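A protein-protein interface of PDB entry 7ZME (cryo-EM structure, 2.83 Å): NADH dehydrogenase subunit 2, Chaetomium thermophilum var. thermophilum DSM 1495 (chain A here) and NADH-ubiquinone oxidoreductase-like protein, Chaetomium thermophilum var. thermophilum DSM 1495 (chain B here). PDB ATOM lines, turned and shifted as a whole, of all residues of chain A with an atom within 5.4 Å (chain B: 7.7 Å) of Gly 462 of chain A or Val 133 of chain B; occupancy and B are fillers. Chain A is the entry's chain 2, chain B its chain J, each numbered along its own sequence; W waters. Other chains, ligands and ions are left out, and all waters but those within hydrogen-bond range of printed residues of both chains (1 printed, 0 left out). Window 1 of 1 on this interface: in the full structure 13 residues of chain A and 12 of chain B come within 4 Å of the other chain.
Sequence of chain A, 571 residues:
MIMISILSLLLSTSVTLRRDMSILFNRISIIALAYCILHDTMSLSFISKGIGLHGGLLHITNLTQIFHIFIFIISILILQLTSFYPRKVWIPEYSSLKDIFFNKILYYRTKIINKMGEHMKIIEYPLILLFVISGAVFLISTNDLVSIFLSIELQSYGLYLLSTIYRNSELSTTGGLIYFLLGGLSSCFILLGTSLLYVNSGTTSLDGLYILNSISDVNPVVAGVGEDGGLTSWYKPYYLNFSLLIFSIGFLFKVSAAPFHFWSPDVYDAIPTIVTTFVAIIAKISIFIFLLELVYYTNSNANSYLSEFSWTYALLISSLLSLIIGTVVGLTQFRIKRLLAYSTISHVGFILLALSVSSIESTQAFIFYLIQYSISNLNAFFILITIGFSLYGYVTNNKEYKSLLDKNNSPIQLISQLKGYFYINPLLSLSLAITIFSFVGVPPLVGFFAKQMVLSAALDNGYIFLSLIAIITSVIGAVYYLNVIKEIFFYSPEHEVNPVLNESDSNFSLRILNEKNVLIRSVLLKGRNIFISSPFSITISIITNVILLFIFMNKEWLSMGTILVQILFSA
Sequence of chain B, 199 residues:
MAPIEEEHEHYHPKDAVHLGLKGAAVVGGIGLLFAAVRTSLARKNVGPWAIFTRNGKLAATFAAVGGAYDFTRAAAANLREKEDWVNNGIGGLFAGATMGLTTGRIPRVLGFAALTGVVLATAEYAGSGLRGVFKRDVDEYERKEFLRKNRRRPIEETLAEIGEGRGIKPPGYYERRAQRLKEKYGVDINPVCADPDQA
Val 133 of chain B touches just these residues of chain A: Asn 461, Gly 462 and Tyr 463.
Printed residues of chain A within 4 Å of Ala 126 of chain B: Ile 464 (3.99 Å).
Printed residues of chain B within 4 Å of Phe 465 of chain A: Ser 128 (3.9 Å).
Printed residues of chain B within 4 Å of Tyr 463 of chain A: Val 133 (3.7 Å).
Arg 136 of chain B touches none of the printed residues of chain A.
Arg 131 of chain B touches none of the printed residues of chain A.
Among the printed residues, 6 pairs touch across the chains.
Among the printed residues, no Asp or Glu carboxylate lies within 4 Å of a Lys or Arg side-chain nitrogen of the other chain.
Among the printed residues, pairs that only touch across the chains: Asn 461 of chain A with Val 133 of chain B (3.6 Å), Asn 303 of chain A with Lys 135 of chain B (3.7 Å), Tyr 463 of chain A with Val 133 of chain B (3.7 Å), Gly 462 of chain A with Val 133 of chain B (3.8 Å), Phe 465 of chain A with Ser 128 of chain B (3.9 Å) and Ile 464 of chain A with Ala 126 of chain B (3.99 Å).
Water W1 bridges N of Phe 465 of chain A (3.2 Å) and N of Gly 129 of chain B (3.4 Å).
The backbone NH (N) of Tyr 463 of chain A lies within hydrogen-bond range of the backbone carbonyl oxygen (O) of Ala 458 of chain A.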
ATOM      1  N   ASN A 303     -31.979   1.330   8.705  1.00  0.00           N
ATOM      2  CA  ASN A 303     -31.054   0.208   8.618  1.00  0.00           C
ATOM      3  C   ASN A 303     -31.744  -1.004   8.006  1.00  0.00           C
ATOM      4  O   ASN A 303     -32.846  -1.380   8.415  1.00  0.00           O
ATOM      5  CB  ASN A 303     -30.506  -0.133  10.003  1.00  0.00           C
ATOM      6  CG  ASN A 303     -29.472   0.867  10.480  1.00  0.00           C
ATOM      7  OD1 ASN A 303     -29.426   2.001  10.006  1.00  0.00           O
ATOM      8  ND2 ASN A 303     -28.634   0.448  11.420  1.00  0.00           N
ATOM      9  N   ALA A 458     -16.974  12.396  15.513  1.00  0.00           N
ATOM     10  CA  ALA A 458     -16.867  10.932  15.441  1.00  0.00           C
ATOM     11  C   ALA A 458     -17.125  10.401  16.841  1.00  0.00           C
ATOM     12  O   ALA A 458     -17.732   9.337  16.950  1.00  0.00           O
ATOM     13  CB  ALA A 458     -15.486  10.583  14.963  1.00  0.00           C
ATOM     14  N   LEU A 459     -16.730  11.153  17.867  1.00  0.00           N
ATOM     15  CA  LEU A 459     -17.037  10.723  19.255  1.00  0.00           C
ATOM     16  C   LEU A 459     -18.552  10.709  19.448  1.00  0.00           C
ATOM     17  O   LEU A 459     -19.061   9.734  20.016  1.00  0.00           O
ATOM     18  CB  LEU A 459     -16.374  11.678  20.248  1.00  0.00           C
ATOM     19  CG  LEU A 459     -14.929  11.376  20.632  1.00  0.00           C
ATOM     20  CD1 LEU A 459     -14.379  12.487  21.507  1.00  0.00           C
ATOM     21  CD2 LEU A 459     -14.820  10.039  21.343  1.00  0.00           C
ATOM     22  N   ASP A 460     -19.240  11.743  18.953  1.00  0.00           N
ATOM     23  CA  ASP A 460     -20.709  11.879  19.145  1.00  0.00           C
ATOM     24  C   ASP A 460     -21.499  10.852  18.339  1.00  0.00           C
ATOM     25  O   ASP A 460     -22.697  10.708  18.607  1.00  0.00           O
ATOM     26  CB  ASP A 460     -21.164  13.289  18.782  1.00  0.00           C
ATOM     27  CG  ASP A 460     -22.281  13.811  19.670  1.00  0.00           C
ATOM     28  OD1 ASP A 460     -22.613  13.129  20.658  1.00  0.00           O
ATOM     29  OD2 ASP A 460     -22.806  14.901  19.368  1.00  0.00           O
ATOM     30  N   ASN A 461     -20.863  10.160  17.401  1.00  0.00           N
ATOM     31  CA  ASN A 461     -21.618   9.231  16.528  1.00  0.00           C
ATOM     32  C   ASN A 461     -21.215   7.781  16.788  1.00  0.00           C
ATOM     33  O   ASN A 461     -21.601   6.926  15.982  1.00  0.00           O
ATOM     34  CB  ASN A 461     -21.613   9.664  15.064  1.00  0.00           C
ATOM     35  CG  ASN A 461     -22.894  10.353  14.648  1.00  0.00           C
ATOM     36  OD1 ASN A 461     -23.475  11.112  15.418  1.00  0.00           O
ATOM     37  ND2 ASN A 461     -23.339  10.099  13.430  1.00  0.00           N
ATOM     38  N   GLY A 462     -20.462   7.521  17.852  1.00  0.00           N
ATOM     39  CA  GLY A 462     -20.139   6.133  18.224  1.00  0.00           C
ATOM     40  C   GLY A 462     -18.933   5.573  17.500  1.00  0.00           C
ATOM     41  O   GLY A 462     -18.670   4.374  17.655  1.00  0.00           O
ATOM     42  N   TYR A 463     -18.232   6.399  16.729  1.00  0.00           N
ATOM     43  CA  TYR A 463     -16.987   5.947  16.064  1.00  0.00           C
ATOM     44  C   TYR A 463     -15.865   6.155  17.076  1.00  0.00           C
ATOM     45  O   TYR A 463     -14.931   6.917  16.794  1.00  0.00           O
ATOM     46  CB  TYR A 463     -16.794   6.717  14.758  1.00  0.00           C
ATOM     47  CG  TYR A 463     -17.859   6.524  13.709  1.00  0.00           C
ATOM     48  CD1 TYR A 463     -19.072   7.184  13.792  1.00  0.00           C
ATOM     49  CD2 TYR A 463     -17.638   5.712  12.612  1.00  0.00           C
ATOM     50  CE1 TYR A 463     -20.049   7.021  12.826  1.00  0.00           C
ATOM     51  CE2 TYR A 463     -18.602   5.543  11.633  1.00  0.00           C
ATOM     52  CZ  TYR A 463     -19.813   6.201  11.740  1.00  0.00           C
ATOM     53  OH  TYR A 463     -20.775   6.044  10.786  1.00  0.00           O
ATOM     54  N   ILE A 464     -15.961   5.485  18.221  1.00  0.00           N
ATOM     55  CA  ILE A 464     -14.973   5.661  19.319  1.00  0.00           C
ATOM     56  C   ILE A 464     -13.671   4.979  18.926  1.00  0.00           C
ATOM     57  O   ILE A 464     -12.613   5.518  19.253  1.00  0.00           O
ATOM     58  CB  ILE A 464     -15.539   5.080  20.631  1.00  0.00           C
ATOM     59  CG1 ILE A 464     -16.987   5.514  20.866  1.00  0.00           C
ATOM     60  CG2 ILE A 464     -14.649   5.424  21.816  1.00  0.00           C
ATOM     61  CD1 ILE A 464     -17.160   7.003  21.039  1.00  0.00           C
ATOM     62  N   PHE A 465     -13.765   3.834  18.255  1.00  0.00           N
ATOM     63  CA  PHE A 465     -12.546   3.088  17.962  1.00  0.00           C
ATOM     64  C   PHE A 465     -11.665   3.831  16.964  1.00  0.00           C
ATOM     65  O   PHE A 465     -10.440   3.866  17.119  1.00  0.00           O
ATOM     66  CB  PHE A 465     -12.914   1.693  17.454  1.00  0.00           C
ATOM     67  CG  PHE A 465     -11.736   0.818  17.153  1.00  0.00           C
ATOM     68  CD1 PHE A 465     -11.121   0.098  18.159  1.00  0.00           C
ATOM     69  CD2 PHE A 465     -11.260   0.694  15.860  1.00  0.00           C
ATOM     70  CE1 PHE A 465     -10.043  -0.713  17.885  1.00  0.00           C
ATOM     71  CE2 PHE A 465     -10.183  -0.114  15.583  1.00  0.00           C
ATOM     72  CZ  PHE A 465      -9.574  -0.819  16.595  1.00  0.00           C
ATOM     73  N   ALA B 126     -16.749  -0.825  22.099  1.00  0.00           N
ATOM     74  CA  ALA B 126     -17.154   0.378  21.390  1.00  0.00           C
ATOM     75  C   ALA B 126     -18.111   0.084  20.245  1.00  0.00           C
ATOM     76  O   ALA B 126     -18.897   0.962  19.871  1.00  0.00           O
ATOM     77  CB  ALA B 126     -15.925   1.117  20.857  1.00  0.00           C
ATOM     78  N   GLY B 127     -18.069  -1.123  19.686  1.00  0.00           N
ATOM     79  CA  GLY B 127     -18.858  -1.425  18.512  1.00  0.00           C
ATOM     80  C   GLY B 127     -18.386  -0.610  17.329  1.00  0.00           C
ATOM     81  O   GLY B 127     -19.097   0.287  16.866  1.00  0.00           O
ATOM     82  N   SER B 128     -17.177  -0.902  16.849  1.00  0.00           N
ATOM     83  CA  SER B 128     -16.559  -0.093  15.806  1.00  0.00           C
ATOM     84  C   SER B 128     -17.456  -0.020  14.578  1.00  0.00           C
ATOM     85  O   SER B 128     -17.957  -1.039  14.097  1.00  0.00           O
ATOM     86  CB  SER B 128     -15.193  -0.668  15.431  1.00  0.00           C
ATOM     87  OG  SER B 128     -15.329  -1.886  14.723  1.00  0.00           O
ATOM     88  N   GLY B 129     -17.647   1.193  14.071  1.00  0.00           N
ATOM     89  CA  GLY B 129     -18.594   1.432  13.002  1.00  0.00           C
ATOM     90  C   GLY B 129     -18.103   1.041  11.626  1.00  0.00           C
ATOM     91  O   GLY B 129     -18.574   1.589  10.625  1.00  0.00           O
ATOM     92  N   LEU B 130     -17.165   0.091  11.558  1.00  0.00           N
ATOM     93  CA  LEU B 130     -16.637  -0.338  10.267  1.00  0.00           C
ATOM     94  C   LEU B 130     -17.739  -0.914   9.388  1.00  0.00           C
ATOM     95  O   LEU B 130     -17.802  -0.625   8.187  1.00  0.00           O
ATOM     96  CB  LEU B 130     -15.520  -1.365  10.465  1.00  0.00           C
ATOM     97  CG  LEU B 130     -14.099  -0.864  10.754  1.00  0.00           C
ATOM     98  CD1 LEU B 130     -13.561  -0.035   9.594  1.00  0.00           C
ATOM     99  CD2 LEU B 130     -14.017  -0.087  12.058  1.00  0.00           C
ATOM    100  N   ARG B 131     -18.617  -1.731   9.966  1.00  0.00           N
ATOM    101  CA  ARG B 131     -19.793  -2.237   9.276  1.00  0.00           C
ATOM    102  C   ARG B 131     -21.030  -1.386   9.546  1.00  0.00           C
ATOM    103  O   ARG B 131     -22.109  -1.693   9.031  1.00  0.00           O
ATOM    104  CB  ARG B 131     -20.047  -3.697   9.683  1.00  0.00           C
ATOM    105  CG  ARG B 131     -21.002  -4.467   8.780  1.00  0.00           C
ATOM    106  CD  ARG B 131     -20.462  -4.586   7.364  1.00  0.00           C
ATOM    107  NE  ARG B 131     -19.545  -5.712   7.212  1.00  0.00           N
ATOM    108  CZ  ARG B 131     -18.806  -5.930   6.131  1.00  0.00           C
ATOM    109  NH1 ARG B 131     -18.000  -6.980   6.076  1.00  0.00           N
ATOM    110  NH2 ARG B 131     -18.871  -5.095   5.103  1.00  0.00           N
ATOM    111  N   GLY B 132     -20.870  -0.312  10.327  1.00  0.00           N
ATOM    112  CA  GLY B 132     -21.980   0.637  10.565  1.00  0.00           C
ATOM    113  C   GLY B 132     -22.361   0.741  12.031  1.00  0.00           C
ATOM    114  O   GLY B 132     -22.518  -0.314  12.674  1.00  0.00           O
ATOM    115  N   VAL B 133     -22.510   1.971  12.539  1.00  0.00           N
ATOM    116  CA  VAL B 133     -22.805   2.204  13.986  1.00  0.00           C
ATOM    117  C   VAL B 133     -24.289   1.976  14.282  1.00  0.00           C
ATOM    118  O   VAL B 133     -25.080   1.902  13.321  1.00  0.00           O
ATOM    119  CB  VAL B 133     -22.355   3.607  14.437  1.00  0.00           C
ATOM    120  CG1 VAL B 133     -20.845   3.710  14.581  1.00  0.00           C
ATOM    121  CG2 VAL B 133     -22.890   4.692  13.514  1.00  0.00           C
ATOM    122  N   PHE B 134     -24.642   1.871  15.566  1.00  0.00           N
ATOM    123  CA  PHE B 134     -26.050   1.612  15.970  1.00  0.00           C
ATOM    124  C   PHE B 134     -26.976   2.759  15.557  1.00  0.00           C
ATOM    125  O   PHE B 134     -26.524   3.921  15.546  1.00  0.00           O
ATOM    126  CB  PHE B 134     -26.130   1.386  17.481  1.00  0.00           C
ATOM    127  N   LYS B 135     -28.236   2.443  15.243  1.00  0.00           N
ATOM    128  CA  LYS B 135     -29.229   3.442  14.874  1.00  0.00           C
ATOM    129  C   LYS B 135     -30.077   3.775  16.095  1.00  0.00           C
ATOM    130  O   LYS B 135     -30.692   2.883  16.692  1.00  0.00           O
ATOM    131  CB  LYS B 135     -30.105   2.937  13.728  1.00  0.00           C
ATOM    132  N   ARG B 136     -30.102   5.056  16.469  1.00  0.00           N
ATOM    133  CA  ARG B 136     -30.855   5.469  17.649  1.00  0.00           C
ATOM    134  C   ARG B 136     -32.350   5.245  17.462  1.00  0.00           C
ATOM    135  O   ARG B 136     -33.035   4.785  18.384  1.00  0.00           O
ATOM    136  CB  ARG B 136     -30.566   6.936  17.966  1.00  0.00           C
HETATM  137  O   HOH W   1     -15.075   2.930  15.473  1.00  0.00           O
